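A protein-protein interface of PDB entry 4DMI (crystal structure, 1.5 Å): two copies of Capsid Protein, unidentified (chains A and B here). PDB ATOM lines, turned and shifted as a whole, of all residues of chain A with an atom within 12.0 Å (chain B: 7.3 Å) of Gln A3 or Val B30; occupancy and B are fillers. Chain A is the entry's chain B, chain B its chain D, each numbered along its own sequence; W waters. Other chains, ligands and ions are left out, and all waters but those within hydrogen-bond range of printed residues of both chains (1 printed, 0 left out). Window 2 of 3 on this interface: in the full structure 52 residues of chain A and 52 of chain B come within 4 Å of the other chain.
O of Thr A36 is in hydrogen-bond range of N of Ser B33 (3.0 Å). The side-chain hydroxyl of Ser B33 lies within hydrogen-bond range of the side-chain hydroxyl of Thr A37, at 2.6 Å. The backbone NH (N) of Ile A38 lies within hydrogen-bond range of the backbone carbonyl oxygen (O) of Ser B33.
OG1 of Thr A37 lies within hydrogen-bond range of OG of Ser A2, 2.8 Å away. The backbone carbonyl oxygen (O) of Gln A3 lies within hydrogen-bond range of the side-chain hydroxyl (OG1) of Thr A36, 2.7 Å away. The side-chain hydroxyl (OG) of Ser A35 lies within hydrogen-bond range of the backbone NH (N) of Thr A37 (3.4 Å). The backbone NH (N) of Ile B7 is in hydrogen-bond range of the backbone carbonyl oxygen (O) of Leu B32 (3.0 Å). The guanidinium group (NE) of Arg B13 sits at hydrogen-bond distance from the backbone carbonyl oxygen (O) of Val B30, 3.5 Å away. The side-chain amide oxygen (OD1) of Asn B17 sits close to the guanidinium group (NE) of Arg B25, 3.1 Å away.
Gln A3 touches Val B30 (NE2 to CB, 3.9 Å). Phe A5 touches Arg B25 (CE1 to NH2, 3.4 Å). Leu B32 touches Thr A36 (CD2 to O, 3.4 Å). Ile A38 touches Ile B7 (CD1 to CD1, 3.6 Å).
Of chain B, only Val B30 (3.9 Å) comes within 4 Å of Gln A3. Printed residues of chain A within 4 Å of Val B30: Gln A3. No residue of chain A comes within 4 Å of Arg B13. No residue of chain A comes within 4 Å of Asp B31. Printed residues of chain B within 4 Å of Thr A37: Ser B33. Printed residues of chain B within 4 Å of Ile A38: Ile B7 and Ser B33. Printed residues of chain B within 4 Å of Thr A36: Leu B32 (3.4 Å) and Ser B33 (3.0 Å). Of the printed residues of chain A, Arg B25 touches Phe A5 (3.4 Å). Of the printed residues of chain A, Ile B7 touches Ile A38 (3.6 Å). Gln A4 touches none of the printed residues of chain B. Ser A2 touches none of the printed residues of chain B. The nearest residue of chain B that does not touch Gln A3 is Asp B31 (5.5 Å). The nearest residue of chain A that does not touch Val B30 is Thr A36 (5.2 Å).
Of the 8 printed residues of chain B, 5 touch a printed residue of chain A. Printed residues of chain B that touch a printed residue of chain A: Ile B7, Arg B25, Val B30, Leu B32 and Ser B33. Of the 15 printed residues of chain A, 5 touch a printed residue of chain B. Among the printed residues, 7 pairs touch across the chains. Among the printed residues, no Asp or Glu carboxylate lies within 4 Å of a Lys or Arg side-chain nitrogen of the other chain.
Positions printed for both chains: 7, 32 and 33.
Water W1 lies within hydrogen-bond range of the side-chain hydroxyl (OG) of Ser B33 (2.7 Å), the side-chain hydroxyl (OG1) of Thr A36 (2.9 Å) and the backbone carbonyl oxygen (O) of Asp B31 (3.2 Å).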
ATOM      1  N   ALA A   1       6.540 -13.841  -1.465  1.00  0.00           N
ATOM      2  CA  ALA A   1       7.299 -13.200  -2.531  1.00  0.00           C
ATOM      3  C   ALA A   1       6.423 -12.194  -3.271  1.00  0.00           C
ATOM      4  O   ALA A   1       5.206 -12.371  -3.370  1.00  0.00           O
ATOM      5  CB  ALA A   1       7.839 -14.254  -3.500  1.00  0.00           C
ATOM      6  N   SER A   2       7.030 -11.134  -3.791  1.00  0.00           N
ATOM      7  CA  SER A   2       6.258 -10.188  -4.576  1.00  0.00           C
ATOM      8  C   SER A   2       5.816 -10.872  -5.857  1.00  0.00           C
ATOM      9  O   SER A   2       6.454 -11.817  -6.327  1.00  0.00           O
ATOM     10  CB  SER A   2       7.064  -8.937  -4.887  1.00  0.00           C
ATOM     11  OG  SER A   2       8.078  -9.200  -5.837  1.00  0.00           O
ATOM     12  N   GLN A   3       4.709 -10.395  -6.402  1.00  0.00           N
ATOM     13  CA  GLN A   3       4.072 -10.993  -7.564  1.00  0.00           C
ATOM     14  C   GLN A   3       5.024 -11.115  -8.756  1.00  0.00           C
ATOM     15  O   GLN A   3       5.773 -10.185  -9.070  1.00  0.00           O
ATOM     16  CB  GLN A   3       2.859 -10.142  -7.919  1.00  0.00           C
ATOM     17  CG  GLN A   3       2.067 -10.576  -9.115  1.00  0.00           C
ATOM     18  CD  GLN A   3       1.007  -9.547  -9.458  1.00  0.00           C
ATOM     19  OE1 GLN A   3       0.659  -8.707  -8.628  1.00  0.00           O
ATOM     20  NE2 GLN A   3       0.504  -9.593 -10.682  1.00  0.00           N
ATOM     21  N   GLN A   4       5.007 -12.279  -9.395  1.00  0.00           N
ATOM     22  CA  GLN A   4       5.852 -12.561 -10.545  1.00  0.00           C
ATOM     23  C   GLN A   4       4.999 -12.799 -11.782  1.00  0.00           C
ATOM     24  O   GLN A   4       3.806 -13.079 -11.679  1.00  0.00           O
ATOM     25  CB  GLN A   4       6.725 -13.789 -10.265  1.00  0.00           C
ATOM     26  CG  GLN A   4       7.738 -13.578  -9.140  1.00  0.00           C
ATOM     27  CD  GLN A   4       8.524 -14.837  -8.813  1.00  0.00           C
ATOM     28  OE1 GLN A   4       8.410 -15.847  -9.504  1.00  0.00           O
ATOM     29  NE2 GLN A   4       9.327 -14.780  -7.755  1.00  0.00           N
ATOM     30  N   PHE A   5       5.617 -12.680 -12.953  1.00  0.00           N
ATOM     31  CA  PHE A   5       4.937 -12.908 -14.223  1.00  0.00           C
ATOM     32  C   PHE A   5       5.804 -13.768 -15.137  1.00  0.00           C
ATOM     33  O   PHE A   5       7.030 -13.738 -15.045  1.00  0.00           O
ATOM     34  CB  PHE A   5       4.619 -11.568 -14.899  1.00  0.00           C
ATOM     35  CG  PHE A   5       5.805 -10.643 -15.006  1.00  0.00           C
ATOM     36  CD1 PHE A   5       6.648 -10.696 -16.109  1.00  0.00           C
ATOM     37  CD2 PHE A   5       6.073  -9.718 -14.007  1.00  0.00           C
ATOM     38  CE1 PHE A   5       7.741  -9.847 -16.210  1.00  0.00           C
ATOM     39  CE2 PHE A   5       7.167  -8.861 -14.099  1.00  0.00           C
ATOM     40  CZ  PHE A   5       7.999  -8.926 -15.203  1.00  0.00           C
ATOM     41  N   ARG A   6       5.171 -14.540 -16.013  1.00  0.00           N
ATOM     42  CA  ARG A   6       5.913 -15.344 -16.975  1.00  0.00           C
ATOM     43  C   ARG A   6       6.466 -14.455 -18.082  1.00  0.00           C
ATOM     44  O   ARG A   6       5.760 -13.597 -18.608  1.00  0.00           O
ATOM     45  CB  ARG A   6       5.027 -16.445 -17.566  1.00  0.00           C
ATOM     46  CG  ARG A   6       5.637 -17.138 -18.779  1.00  0.00           C
ATOM     47  CD  ARG A   6       4.960 -18.472 -19.092  1.00  0.00           C
ATOM     48  NE  ARG A   6       5.258 -19.471 -18.069  1.00  0.00           N
ATOM     49  CZ  ARG A   6       4.423 -19.818 -17.096  1.00  0.00           C
ATOM     50  NH1 ARG A   6       3.221 -19.263 -17.025  1.00  0.00           N
ATOM     51  NH2 ARG A   6       4.785 -20.725 -16.198  1.00  0.00           N
ATOM     52  N   ILE A   7       7.739 -14.639 -18.417  1.00  0.00           N
ATOM     53  CA  ILE A   7       8.346 -13.871 -19.502  1.00  0.00           C
ATOM     54  C   ILE A   7       8.320 -14.671 -20.796  1.00  0.00           C
ATOM     55  O   ILE A   7       8.784 -15.812 -20.848  1.00  0.00           O
ATOM     56  CB  ILE A   7       9.786 -13.468 -19.164  1.00  0.00           C
ATOM     57  CG1 ILE A   7       9.792 -12.468 -18.008  1.00  0.00           C
ATOM     58  CG2 ILE A   7      10.476 -12.871 -20.387  1.00  0.00           C
ATOM     59  CD1 ILE A   7      11.162 -12.238 -17.402  1.00  0.00           C
ATOM     60  N   LEU A  32      11.162 -18.789 -17.851  1.00  0.00           N
ATOM     61  CA  LEU A  32      11.522 -17.517 -17.233  1.00  0.00           C
ATOM     62  C   LEU A  32      10.362 -16.798 -16.564  1.00  0.00           C
ATOM     63  O   LEU A  32       9.257 -16.730 -17.102  1.00  0.00           O
ATOM     64  CB  LEU A  32      12.121 -16.571 -18.271  1.00  0.00           C
ATOM     65  CG  LEU A  32      13.533 -16.844 -18.778  1.00  0.00           C
ATOM     66  CD1 LEU A  32      13.820 -15.950 -19.963  1.00  0.00           C
ATOM     67  CD2 LEU A  32      14.535 -16.596 -17.671  1.00  0.00           C
ATOM     68  N   SER A  33      10.631 -16.254 -15.385  1.00  0.00           N
ATOM     69  CA  SER A  33       9.693 -15.346 -14.747  1.00  0.00           C
ATOM     70  C   SER A  33      10.392 -14.027 -14.456  1.00  0.00           C
ATOM     71  O   SER A  33      11.624 -13.957 -14.454  1.00  0.00           O
ATOM     72  CB  SER A  33       9.116 -15.965 -13.469  1.00  0.00           C
ATOM     73  OG  SER A  33      10.139 -16.354 -12.567  1.00  0.00           O
ATOM     74  N   GLY A  34       9.604 -12.976 -14.247  1.00  0.00           N
ATOM     75  CA  GLY A  34      10.136 -11.697 -13.810  1.00  0.00           C
ATOM     76  C   GLY A  34       9.482 -11.259 -12.511  1.00  0.00           C
ATOM     77  O   GLY A  34       8.320 -11.587 -12.254  1.00  0.00           O
ATOM     78  N   SER A  35      10.231 -10.534 -11.686  1.00  0.00           N
ATOM     79  CA  SER A  35       9.714 -10.028 -10.413  1.00  0.00           C
ATOM     80  C   SER A  35       9.204  -8.593 -10.546  1.00  0.00           C
ATOM     81  O   SER A  35       9.707  -7.818 -11.365  1.00  0.00           O
ATOM     82  CB  SER A  35      10.801 -10.098  -9.338  1.00  0.00           C
ATOM     83  OG  SER A  35      10.332  -9.584  -8.098  1.00  0.00           O
ATOM     84  N   THR A  36       8.216  -8.233  -9.733  1.00  0.00           N
ATOM     85  CA  THR A  36       7.659  -6.882  -9.771  1.00  0.00           C
ATOM     86  C   THR A  36       8.232  -5.949  -8.706  1.00  0.00           C
ATOM     87  O   THR A  36       7.777  -4.815  -8.571  1.00  0.00           O
ATOM     88  CB  THR A  36       6.117  -6.876  -9.654  1.00  0.00           C
ATOM     89  OG1 THR A  36       5.713  -7.541  -8.443  1.00  0.00           O
ATOM     90  CG2 THR A  36       5.474  -7.563 -10.854  1.00  0.00           C
ATOM     91  N   THR A  37       9.213  -6.419  -7.938  1.00  0.00           N
ATOM     92  CA  THR A  37       9.874  -5.545  -6.973  1.00  0.00           C
ATOM     93  C   THR A  37      11.263  -5.143  -7.449  1.00  0.00           C
ATOM     94  O   THR A  37      12.114  -5.994  -7.717  1.00  0.00           O
ATOM     95  CB  THR A  37       9.988  -6.185  -5.589  1.00  0.00           C
ATOM     96  OG1 THR A  37       8.681  -6.512  -5.114  1.00  0.00           O
ATOM     97  CG2 THR A  37      10.624  -5.215  -4.600  1.00  0.00           C
ATOM     98  N   ILE A  38      11.483  -3.835  -7.543  1.00  0.00           N
ATOM     99  CA  ILE A  38      12.771  -3.288  -7.943  1.00  0.00           C
ATOM    100  C   ILE A  38      13.716  -3.263  -6.753  1.00  0.00           C
ATOM    101  O   ILE A  38      13.384  -2.740  -5.683  1.00  0.00           O
ATOM    102  CB  ILE A  38      12.603  -1.877  -8.516  1.00  0.00           C
ATOM    103  CG1 ILE A  38      11.627  -1.926  -9.687  1.00  0.00           C
ATOM    104  CG2 ILE A  38      13.955  -1.287  -8.940  1.00  0.00           C
ATOM    105  CD1 ILE A  38      11.348  -0.583 -10.301  1.00  0.00           C
ATOM    106  N   ILE A  39      14.886  -3.860  -6.941  1.00  0.00           N
ATOM    107  CA  ILE A  39      15.863  -4.008  -5.874  1.00  0.00           C
ATOM    108  C   ILE A  39      17.025  -3.041  -6.080  1.00  0.00           C
ATOM    109  O   ILE A  39      17.639  -3.031  -7.140  1.00  0.00           O
ATOM    110  CB  ILE A  39      16.423  -5.438  -5.857  1.00  0.00           C
ATOM    111  CG1 ILE A  39      15.285  -6.459  -5.752  1.00  0.00           C
ATOM    112  CG2 ILE A  39      17.427  -5.603  -4.716  1.00  0.00           C
ATOM    113  CD1 ILE A  39      14.402  -6.297  -4.521  1.00  0.00           C
ATOM    114  N   ILE B   7       5.591   1.788  -5.881  1.00  0.00           N
ATOM    115  CA  ILE B   7       6.218   2.776  -6.749  1.00  0.00           C
ATOM    116  C   ILE B   7       5.173   3.466  -7.623  1.00  0.00           C
ATOM    117  O   ILE B   7       4.274   2.820  -8.167  1.00  0.00           O
ATOM    118  CB  ILE B   7       7.311   2.127  -7.630  1.00  0.00           C
ATOM    119  CG1 ILE B   7       8.528   1.764  -6.778  1.00  0.00           C
ATOM    120  CG2 ILE B   7       7.728   3.054  -8.776  1.00  0.00           C
ATOM    121  CD1 ILE B   7       9.587   0.984  -7.535  1.00  0.00           C
ATOM    122  N   ARG B  13       7.426   1.527 -15.033  1.00  0.00           N
ATOM    123  CA  ARG B  13       6.532   0.416 -15.349  1.00  0.00           C
ATOM    124  C   ARG B  13       6.541   0.076 -16.842  1.00  0.00           C
ATOM    125  O   ARG B  13       6.622  -1.095 -17.218  1.00  0.00           O
ATOM    126  CB  ARG B  13       5.105   0.723 -14.887  1.00  0.00           C
ATOM    127  CG  ARG B  13       4.109  -0.382 -15.195  1.00  0.00           C
ATOM    128  CD  ARG B  13       2.675   0.130 -15.114  1.00  0.00           C
ATOM    129  NE  ARG B  13       2.090  -0.025 -13.788  1.00  0.00           N
ATOM    130  CZ  ARG B  13       1.018   0.641 -13.369  1.00  0.00           C
ATOM    131  NH1 ARG B  13       0.431   1.521 -14.171  1.00  0.00           N
ATOM    132  NH2 ARG B  13       0.539   0.442 -12.148  1.00  0.00           N
ATOM    133  N   ASN B  17       7.950  -3.381 -18.631  1.00  0.00           N
ATOM    134  CA  ASN B  17       7.049  -4.135 -19.500  1.00  0.00           C
ATOM    135  C   ASN B  17       7.630  -4.398 -20.891  1.00  0.00           C
ATOM    136  O   ASN B  17       7.366  -5.437 -21.498  1.00  0.00           O
ATOM    137  CB  ASN B  17       5.694  -3.429 -19.623  1.00  0.00           C
ATOM    138  CG  ASN B  17       4.824  -3.603 -18.388  1.00  0.00           C
ATOM    139  OD1 ASN B  17       5.107  -4.424 -17.515  1.00  0.00           O
ATOM    140  ND2 ASN B  17       3.741  -2.836 -18.323  1.00  0.00           N
ATOM    141  N   ARG B  25       0.027 -10.637 -19.540  1.00  0.00           N
ATOM    142  CA  ARG B  25      -0.172  -9.285 -19.007  1.00  0.00           C
ATOM    143  C   ARG B  25      -1.364  -8.665 -19.697  1.00  0.00           C
ATOM    144  O   ARG B  25      -1.480  -8.794 -20.894  1.00  0.00           O
ATOM    145  CB  ARG B  25       1.080  -8.431 -19.275  1.00  0.00           C
ATOM    146  CG  ARG B  25       1.136  -7.052 -18.638  1.00  0.00           C
ATOM    147  CD  ARG B  25       2.495  -6.424 -18.858  1.00  0.00           C
ATOM    148  NE  ARG B  25       3.605  -7.077 -18.162  1.00  0.00           N
ATOM    149  CZ  ARG B  25       4.804  -7.258 -18.683  1.00  0.00           C
ATOM    150  NH1 ARG B  25       5.035  -6.908 -19.905  1.00  0.00           N
ATOM    151  NH2 ARG B  25       5.734  -7.797 -17.978  1.00  0.00           N
ATOM    152  N   VAL B  30      -0.380  -4.006 -13.074  1.00  0.00           N
ATOM    153  CA  VAL B  30       0.027  -4.419 -11.735  1.00  0.00           C
ATOM    154  C   VAL B  30       0.959  -3.398 -11.075  1.00  0.00           C
ATOM    155  O   VAL B  30       1.821  -2.811 -11.734  1.00  0.00           O
ATOM    156  CB  VAL B  30       0.684  -5.824 -11.763  1.00  0.00           C
ATOM    157  N   ASP B  31       0.765  -3.178  -9.778  1.00  0.00           N
ATOM    158  CA  ASP B  31       1.610  -2.273  -9.008  1.00  0.00           C
ATOM    159  C   ASP B  31       3.045  -2.771  -8.893  1.00  0.00           C
ATOM    160  O   ASP B  31       3.296  -3.882  -8.427  1.00  0.00           O
ATOM    161  CB  ASP B  31       1.034  -2.049  -7.607  1.00  0.00           C
ATOM    162  N   LEU B  32       3.984  -1.938  -9.328  1.00  0.00           N
ATOM    163  CA  LEU B  32       5.391  -2.199  -9.083  1.00  0.00           C
ATOM    164  C   LEU B  32       5.733  -1.795  -7.657  1.00  0.00           C
ATOM    165  O   LEU B  32       5.096  -0.911  -7.076  1.00  0.00           O
ATOM    166  CB  LEU B  32       6.272  -1.432 -10.068  1.00  0.00           C
ATOM    167  CG  LEU B  32       6.314  -1.973 -11.496  1.00  0.00           C
ATOM    168  CD1 LEU B  32       7.410  -1.286 -12.300  1.00  0.00           C
ATOM    169  CD2 LEU B  32       6.505  -3.486 -11.487  1.00  0.00           C
ATOM    170  N   SER B  33       6.733  -2.452  -7.086  1.00  0.00           N
ATOM    171  CA  SER B  33       7.172  -2.109  -5.745  1.00  0.00           C
ATOM    172  C   SER B  33       8.679  -1.927  -5.702  1.00  0.00           C
ATOM    173  O   SER B  33       9.385  -2.286  -6.644  1.00  0.00           O
ATOM    174  CB  SER B  33       6.718  -3.164  -4.729  1.00  0.00           C
ATOM    175  OG  SER B  33       7.076  -4.473  -5.140  1.00  0.00           O
HETATM  176  O   HOH W   1       5.008  -5.647  -6.428  1.00  0.00           O
